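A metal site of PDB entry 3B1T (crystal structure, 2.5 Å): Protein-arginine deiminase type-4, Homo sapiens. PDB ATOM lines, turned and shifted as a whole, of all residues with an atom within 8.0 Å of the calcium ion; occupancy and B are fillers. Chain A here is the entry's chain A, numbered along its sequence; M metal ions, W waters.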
ATOM      1  N   ASP A 358     -16.410 -25.847 -34.792  1.00  0.00           N
ATOM      2  CA  ASP A 358     -16.207 -24.482 -34.325  1.00  0.00           C
ATOM      3  C   ASP A 358     -16.468 -24.232 -32.824  1.00  0.00           C
ATOM      4  O   ASP A 358     -15.745 -23.442 -32.226  1.00  0.00           O
ATOM      5  CB  ASP A 358     -17.054 -23.534 -35.167  1.00  0.00           C
ATOM      6  CG  ASP A 358     -16.630 -23.531 -36.626  1.00  0.00           C
ATOM      7  OD1 ASP A 358     -15.542 -24.046 -36.964  1.00  0.00           O
ATOM      8  OD2 ASP A 358     -17.393 -22.995 -37.446  1.00  0.00           O
ATOM      9  N   GLU A 359     -17.469 -24.877 -32.225  1.00  0.00           N
ATOM     10  CA  GLU A 359     -17.874 -24.552 -30.859  1.00  0.00           C
ATOM     11  C   GLU A 359     -16.932 -25.156 -29.784  1.00  0.00           C
ATOM     12  O   GLU A 359     -16.813 -24.636 -28.689  1.00  0.00           O
ATOM     13  CB  GLU A 359     -19.344 -24.973 -30.613  1.00  0.00           C
ATOM     14  CG  GLU A 359     -20.005 -24.471 -29.283  1.00  0.00           C
ATOM     15  CD  GLU A 359     -20.409 -22.978 -29.280  1.00  0.00           C
ATOM     16  OE1 GLU A 359     -20.469 -22.371 -28.167  1.00  0.00           O
ATOM     17  OE2 GLU A 359     -20.682 -22.422 -30.370  1.00  0.00           O
ATOM     18  N   MET A 360     -16.250 -26.254 -30.107  1.00  0.00           N
ATOM     19  CA  MET A 360     -15.426 -26.907 -29.105  1.00  0.00           C
ATOM     20  C   MET A 360     -14.130 -27.497 -29.668  1.00  0.00           C
ATOM     21  O   MET A 360     -13.960 -27.645 -30.879  1.00  0.00           O
ATOM     22  CB  MET A 360     -16.255 -28.007 -28.445  1.00  0.00           C
ATOM     23  CG  MET A 360     -16.480 -29.181 -29.354  1.00  0.00           C
ATOM     24  SD  MET A 360     -17.436 -30.520 -28.634  1.00  0.00           S
ATOM     25  CE  MET A 360     -17.226 -31.710 -29.957  1.00  0.00           C
ATOM     26  N   PHE A 376     -12.676 -27.960 -24.394  1.00  0.00           N
ATOM     27  CA  PHE A 376     -12.453 -26.563 -24.308  1.00  0.00           C
ATOM     28  C   PHE A 376     -13.541 -25.992 -25.195  1.00  0.00           C
ATOM     29  O   PHE A 376     -13.529 -26.203 -26.410  1.00  0.00           O
ATOM     30  CB  PHE A 376     -11.037 -26.237 -24.770  1.00  0.00           C
ATOM     31  CG  PHE A 376     -10.690 -24.780 -24.746  1.00  0.00           C
ATOM     32  CD1 PHE A 376     -11.311 -23.905 -23.854  1.00  0.00           C
ATOM     33  CD2 PHE A 376      -9.731 -24.285 -25.591  1.00  0.00           C
ATOM     34  CE1 PHE A 376     -10.974 -22.551 -23.835  1.00  0.00           C
ATOM     35  CE2 PHE A 376      -9.384 -22.914 -25.566  1.00  0.00           C
ATOM     36  CZ  PHE A 376     -10.002 -22.070 -24.696  1.00  0.00           C
ATOM     37  N   ASP A 377     -14.487 -25.303 -24.568  1.00  0.00           N
ATOM     38  CA  ASP A 377     -15.713 -24.819 -25.202  1.00  0.00           C
ATOM     39  C   ASP A 377     -15.572 -23.354 -25.593  1.00  0.00           C
ATOM     40  O   ASP A 377     -15.378 -22.475 -24.760  1.00  0.00           O
ATOM     41  CB  ASP A 377     -16.883 -24.995 -24.224  1.00  0.00           C
ATOM     42  CG  ASP A 377     -18.163 -24.303 -24.677  1.00  0.00           C
ATOM     43  OD1 ASP A 377     -18.319 -23.948 -25.870  1.00  0.00           O
ATOM     44  OD2 ASP A 377     -19.029 -24.111 -23.793  1.00  0.00           O
ATOM     45  N   SER A 378     -15.696 -23.098 -26.897  1.00  0.00           N
ATOM     46  CA  SER A 378     -15.484 -21.771 -27.454  1.00  0.00           C
ATOM     47  C   SER A 378     -16.587 -20.783 -27.051  1.00  0.00           C
ATOM     48  O   SER A 378     -17.767 -21.150 -27.015  1.00  0.00           O
ATOM     49  CB  SER A 378     -15.445 -21.870 -28.979  1.00  0.00           C
ATOM     50  OG  SER A 378     -15.178 -20.622 -29.574  1.00  0.00           O
ATOM     51  N   PRO A 379     -16.209 -19.519 -26.788  1.00  0.00           N
ATOM     52  CA  PRO A 379     -17.189 -18.482 -26.482  1.00  0.00           C
ATOM     53  C   PRO A 379     -18.068 -18.070 -27.668  1.00  0.00           C
ATOM     54  O   PRO A 379     -18.940 -17.216 -27.501  1.00  0.00           O
ATOM     55  CB  PRO A 379     -16.309 -17.288 -26.075  1.00  0.00           C
ATOM     56  CG  PRO A 379     -15.089 -17.472 -26.854  1.00  0.00           C
ATOM     57  CD  PRO A 379     -14.842 -18.958 -26.857  1.00  0.00           C
ATOM     58  N   ARG A 380     -17.873 -18.659 -28.847  1.00  0.00           N
ATOM     59  CA  ARG A 380     -18.620 -18.201 -30.003  1.00  0.00           C
ATOM     60  C   ARG A 380     -20.134 -18.313 -29.762  1.00  0.00           C
ATOM     61  O   ARG A 380     -20.903 -17.511 -30.304  1.00  0.00           O
ATOM     62  CB  ARG A 380     -18.150 -18.878 -31.314  1.00  0.00           C
ATOM     63  CG  ARG A 380     -18.667 -20.251 -31.588  1.00  0.00           C
ATOM     64  CD  ARG A 380     -19.119 -20.414 -33.050  1.00  0.00           C
ATOM     65  NE  ARG A 380     -20.059 -21.529 -33.185  1.00  0.00           N
ATOM     66  CZ  ARG A 380     -20.405 -22.117 -34.330  1.00  0.00           C
ATOM     67  NH1 ARG A 380     -19.905 -21.719 -35.496  1.00  0.00           N
ATOM     68  NH2 ARG A 380     -21.264 -23.116 -34.283  1.00  0.00           N
ATOM     69  N   ASN A 381     -20.523 -19.285 -28.930  1.00  0.00           N
ATOM     70  CA  ASN A 381     -21.881 -19.377 -28.371  1.00  0.00           C
ATOM     71  C   ASN A 381     -22.990 -19.210 -29.416  1.00  0.00           C
ATOM     72  O   ASN A 381     -23.851 -18.334 -29.327  1.00  0.00           O
ATOM     73  CB  ASN A 381     -22.041 -18.392 -27.197  1.00  0.00           C
ATOM     74  CG  ASN A 381     -21.238 -18.814 -25.963  1.00  0.00           C
ATOM     75  OD1 ASN A 381     -20.847 -19.982 -25.838  1.00  0.00           O
ATOM     76  ND2 ASN A 381     -20.993 -17.883 -25.057  1.00  0.00           N
ATOM     77  N   ARG A 382     -22.956 -20.106 -30.401  1.00  0.00           N
ATOM     78  CA  ARG A 382     -23.889 -20.100 -31.522  1.00  0.00           C
ATOM     79  C   ARG A 382     -24.996 -21.121 -31.190  1.00  0.00           C
ATOM     80  O   ARG A 382     -25.303 -21.330 -30.016  1.00  0.00           O
ATOM     81  CB  ARG A 382     -23.104 -20.424 -32.807  1.00  0.00           C
ATOM     82  CG  ARG A 382     -23.575 -19.712 -34.068  1.00  0.00           C
ATOM     83  CD  ARG A 382     -22.845 -18.394 -34.374  1.00  0.00           C
ATOM     84  NE  ARG A 382     -21.770 -18.521 -35.369  1.00  0.00           N
ATOM     85  CZ  ARG A 382     -21.924 -18.732 -36.682  1.00  0.00           C
ATOM     86  NH1 ARG A 382     -23.129 -18.890 -37.230  1.00  0.00           N
ATOM     87  NH2 ARG A 382     -20.856 -18.811 -37.469  1.00  0.00           N
ATOM     88  N   LEU A 384     -24.842 -24.427 -31.430  1.00  0.00           N
ATOM     89  CA  LEU A 384     -24.196 -25.578 -30.740  1.00  0.00           C
ATOM     90  C   LEU A 384     -23.842 -25.303 -29.261  1.00  0.00           C
ATOM     91  O   LEU A 384     -23.437 -26.220 -28.555  1.00  0.00           O
ATOM     92  CB  LEU A 384     -22.948 -26.040 -31.502  1.00  0.00           C
ATOM     93  CG  LEU A 384     -22.923 -27.436 -32.147  1.00  0.00           C
ATOM     94  CD1 LEU A 384     -24.225 -28.217 -32.018  1.00  0.00           C
ATOM     95  CD2 LEU A 384     -22.464 -27.344 -33.606  1.00  0.00           C
ATOM     96  N   LYS A 385     -24.025 -24.058 -28.812  1.00  0.00           N
ATOM     97  CA  LYS A 385     -23.608 -23.567 -27.488  1.00  0.00           C
ATOM     98  C   LYS A 385     -23.682 -24.570 -26.321  1.00  0.00           C
ATOM     99  O   LYS A 385     -22.714 -24.714 -25.569  1.00  0.00           O
ATOM    100  CB  LYS A 385     -24.394 -22.289 -27.123  1.00  0.00           C
ATOM    101  CG  LYS A 385     -24.065 -21.677 -25.756  1.00  0.00           C
ATOM    102  CD  LYS A 385     -25.027 -20.528 -25.357  1.00  0.00           C
ATOM    103  CE  LYS A 385     -24.945 -20.235 -23.855  1.00  0.00           C
ATOM    104  NZ  LYS A 385     -25.697 -19.006 -23.476  1.00  0.00           N
ATOM    105  N   GLU A 386     -24.830 -25.217 -26.173  1.00  0.00           N
ATOM    106  CA  GLU A 386     -25.107 -26.066 -24.996  1.00  0.00           C
ATOM    107  C   GLU A 386     -24.420 -27.440 -25.047  1.00  0.00           C
ATOM    108  O   GLU A 386     -24.113 -28.029 -23.989  1.00  0.00           O
ATOM    109  CB  GLU A 386     -26.628 -26.243 -24.801  1.00  0.00           C
ATOM    110  CG  GLU A 386     -27.371 -24.990 -24.306  1.00  0.00           C
ATOM    111  CD  GLU A 386     -26.812 -24.445 -22.992  1.00  0.00           C
ATOM    112  OE1 GLU A 386     -26.677 -23.208 -22.859  1.00  0.00           O
ATOM    113  OE2 GLU A 386     -26.474 -25.251 -22.086  1.00  0.00           O
ATOM    114  N   PHE A 387     -24.166 -27.928 -26.262  1.00  0.00           N
ATOM    115  CA  PHE A 387     -23.617 -29.274 -26.528  1.00  0.00           C
ATOM    116  C   PHE A 387     -22.341 -29.655 -25.728  1.00  0.00           C
ATOM    117  O   PHE A 387     -22.253 -30.779 -25.241  1.00  0.00           O
ATOM    118  CB  PHE A 387     -23.393 -29.459 -28.049  1.00  0.00           C
ATOM    119  CG  PHE A 387     -22.925 -30.839 -28.424  1.00  0.00           C
ATOM    120  CD1 PHE A 387     -23.758 -31.940 -28.244  1.00  0.00           C
ATOM    121  CD2 PHE A 387     -21.662 -31.037 -28.973  1.00  0.00           C
ATOM    122  CE1 PHE A 387     -23.344 -33.216 -28.582  1.00  0.00           C
ATOM    123  CE2 PHE A 387     -21.230 -32.319 -29.325  1.00  0.00           C
ATOM    124  CZ  PHE A 387     -22.075 -33.409 -29.119  1.00  0.00           C
ATOM    125  N   PRO A 388     -21.361 -28.739 -25.612  1.00  0.00           N
ATOM    126  CA  PRO A 388     -20.313 -28.981 -24.627  1.00  0.00           C
ATOM    127  C   PRO A 388     -20.814 -29.105 -23.181  1.00  0.00           C
ATOM    128  O   PRO A 388     -20.353 -29.987 -22.461  1.00  0.00           O
ATOM    129  CB  PRO A 388     -19.403 -27.760 -24.795  1.00  0.00           C
ATOM    130  CG  PRO A 388     -19.503 -27.439 -26.212  1.00  0.00           C
ATOM    131  CD  PRO A 388     -20.962 -27.670 -26.557  1.00  0.00           C
ATOM    132  N   ILE A 389     -21.767 -28.271 -22.767  1.00  0.00           N
ATOM    133  CA  ILE A 389     -22.245 -28.289 -21.378  1.00  0.00           C
ATOM    134  C   ILE A 389     -23.038 -29.581 -21.043  1.00  0.00           C
ATOM    135  O   ILE A 389     -22.716 -30.267 -20.073  1.00  0.00           O
ATOM    136  CB  ILE A 389     -23.094 -27.024 -21.009  1.00  0.00           C
ATOM    137  CG1 ILE A 389     -22.329 -25.735 -21.357  1.00  0.00           C
ATOM    138  CG2 ILE A 389     -23.466 -27.047 -19.513  1.00  0.00           C
ATOM    139  CD1 ILE A 389     -22.936 -24.449 -20.773  1.00  0.00           C
ATOM    140  N   TYR A 399     -14.445 -30.122 -18.529  1.00  0.00           N
ATOM    141  CA  TYR A 399     -14.929 -28.963 -19.234  1.00  0.00           C
ATOM    142  C   TYR A 399     -14.096 -27.720 -18.916  1.00  0.00           C
ATOM    143  O   TYR A 399     -13.564 -27.591 -17.817  1.00  0.00           O
ATOM    144  CB  TYR A 399     -16.389 -28.753 -18.865  1.00  0.00           C
ATOM    145  CG  TYR A 399     -16.951 -27.525 -19.504  1.00  0.00           C
ATOM    146  CD1 TYR A 399     -17.565 -27.591 -20.741  1.00  0.00           C
ATOM    147  CD2 TYR A 399     -16.830 -26.280 -18.880  1.00  0.00           C
ATOM    148  CE1 TYR A 399     -18.064 -26.452 -21.337  1.00  0.00           C
ATOM    149  CE2 TYR A 399     -17.316 -25.142 -19.465  1.00  0.00           C
ATOM    150  CZ  TYR A 399     -17.939 -25.231 -20.689  1.00  0.00           C
ATOM    151  OH  TYR A 399     -18.447 -24.091 -21.274  1.00  0.00           O
ATOM    152  N   VAL A 400     -13.965 -26.825 -19.887  1.00  0.00           N
ATOM    153  CA  VAL A 400     -13.392 -25.495 -19.681  1.00  0.00           C
ATOM    154  C   VAL A 400     -13.906 -24.523 -20.721  1.00  0.00           C
ATOM    155  O   VAL A 400     -14.139 -24.895 -21.871  1.00  0.00           O
ATOM    156  CB  VAL A 400     -11.849 -25.445 -19.901  1.00  0.00           C
ATOM    157  CG1 VAL A 400     -11.245 -24.210 -19.165  1.00  0.00           C
ATOM    158  CG2 VAL A 400     -11.163 -26.722 -19.458  1.00  0.00           C
ATOM    159  N   THR A 401     -13.998 -23.258 -20.338  1.00  0.00           N
ATOM    160  CA  THR A 401     -14.344 -22.210 -21.293  1.00  0.00           C
ATOM    161  C   THR A 401     -13.506 -20.972 -20.999  1.00  0.00           C
ATOM    162  O   THR A 401     -12.926 -20.851 -19.923  1.00  0.00           O
ATOM    163  CB  THR A 401     -15.873 -21.865 -21.206  1.00  0.00           C
ATOM    164  OG1 THR A 401     -16.319 -21.383 -22.476  1.00  0.00           O
ATOM    165  CG2 THR A 401     -16.166 -20.840 -20.127  1.00  0.00           C
ATOM    166  N   ARG A 402     -13.476 -20.038 -21.946  1.00  0.00           N
ATOM    167  CA  ARG A 402     -12.762 -18.768 -21.802  1.00  0.00           C
ATOM    168  C   ARG A 402     -13.394 -17.716 -22.708  1.00  0.00           C
ATOM    169  O   ARG A 402     -13.957 -18.035 -23.739  1.00  0.00           O
ATOM    170  CB  ARG A 402     -11.259 -18.905 -22.144  1.00  0.00           C
ATOM    171  CG  ARG A 402     -10.354 -19.553 -21.086  1.00  0.00           C
ATOM    172  CD  ARG A 402     -10.552 -18.887 -19.751  1.00  0.00           C
ATOM    173  NE  ARG A 402      -9.602 -19.327 -18.734  1.00  0.00           N
ATOM    174  CZ  ARG A 402      -9.769 -20.337 -17.891  1.00  0.00           C
ATOM    175  NH1 ARG A 402     -10.837 -21.109 -17.957  1.00  0.00           N
ATOM    176  NH2 ARG A 402      -8.825 -20.600 -16.980  1.00  0.00           N
ATOM    177  N   GLN A 405     -18.757 -14.271 -22.619  1.00  0.00           N
ATOM    178  CA  GLN A 405     -19.805 -15.210 -22.990  1.00  0.00           C
ATOM    179  C   GLN A 405     -21.057 -14.508 -23.577  1.00  0.00           C
ATOM    180  O   GLN A 405     -21.748 -15.095 -24.409  1.00  0.00           O
ATOM    181  CB  GLN A 405     -20.134 -16.104 -21.777  1.00  0.00           C
ATOM    182  CG  GLN A 405     -18.951 -16.966 -21.303  1.00  0.00           C
ATOM    183  CD  GLN A 405     -18.501 -17.980 -22.365  1.00  0.00           C
ATOM    184  OE1 GLN A 405     -19.335 -18.644 -22.994  1.00  0.00           O
ATOM    185  NE2 GLN A 405     -17.193 -18.071 -22.587  1.00  0.00           N
ATOM    186  N   PHE A 415     -13.262 -22.609 -33.347  1.00  0.00           N
ATOM    187  CA  PHE A 415     -12.186 -23.578 -33.104  1.00  0.00           C
ATOM    188  C   PHE A 415     -11.779 -24.363 -34.318  1.00  0.00           C
ATOM    189  O   PHE A 415     -10.965 -25.278 -34.231  1.00  0.00           O
ATOM    190  CB  PHE A 415     -12.563 -24.467 -31.923  1.00  0.00           C
ATOM    191  CG  PHE A 415     -12.415 -23.779 -30.574  1.00  0.00           C
ATOM    192  CD1 PHE A 415     -12.374 -24.517 -29.416  1.00  0.00           C
ATOM    193  CD2 PHE A 415     -12.264 -22.390 -30.482  1.00  0.00           C
ATOM    194  CE1 PHE A 415     -12.206 -23.903 -28.190  1.00  0.00           C
ATOM    195  CE2 PHE A 415     -12.083 -21.770 -29.264  1.00  0.00           C
ATOM    196  CZ  PHE A 415     -12.065 -22.527 -28.113  1.00  0.00           C
HETATM  197 CA    CA M   1     -19.682 -21.982 -25.979  1.00  0.00          CA
HETATM  198  O   HOH W   1     -18.859 -20.996 -24.074  1.00  0.00           O
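Water W1 lies within hydrogen-bond range of the side-chain amide oxygen (OE1) of Gln 405, the side-chain hydroxyl (OG1) of Thr 401 and the side-chain carboxylate (OD2) of Asp 377.
The nearest printed residue that does not touch the calcium ion is Lys 385 (4.1 Å).
The side-chain amide nitrogen of Asn 381 lies close to the backbone carbonyl oxygen of Pro 379, at 3.3 Å. The side-chain amide nitrogen (ND2) of Asn 381 sits at hydrogen-bond distance from the side-chain amide oxygen (OE1) of Gln 405. The side-chain hydroxyl (OG) of Ser 378 sits close to the backbone NH (N) of Arg 380 (3.4 Å). NE of Arg 380 is in salt-bridge range of OE2 of Glu 359. N of Arg 382 sits at hydrogen-bond distance from OE2 of Glu 359, at 3.2 Å. The backbone carbonyl oxygen (O) of Asp 377 sits at hydrogen-bond distance from the side-chain hydroxyl (OG1) of Thr 401 (2.7 Å). The side-chain carboxylate of Asp 377 sits at hydrogen-bond distance from the side-chain hydroxyl of Tyr 399 (2.6 Å). The backbone carbonyl oxygen (O) of Val 400 lies within hydrogen-bond range of the backbone NH (N) of Asp 377, 2.7 Å away.
The calcium ion is bound by water W1 (2.3 Å), the side-chain amide oxygen (OD1) of Asn 381 (2.3 Å), the backbone carbonyl oxygen (O) of Ser 378 (2.3 Å), the side-chain carboxylate (OE1) of Glu 359 (2.4 Å) and the side-chain carboxylate (OD1) of Asp 377 (2.4 Å). The calcium ion has five donor atoms within binding distance. Slightly farther from the calcium ion lies OD2 of Asp 377 (3.1 Å).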
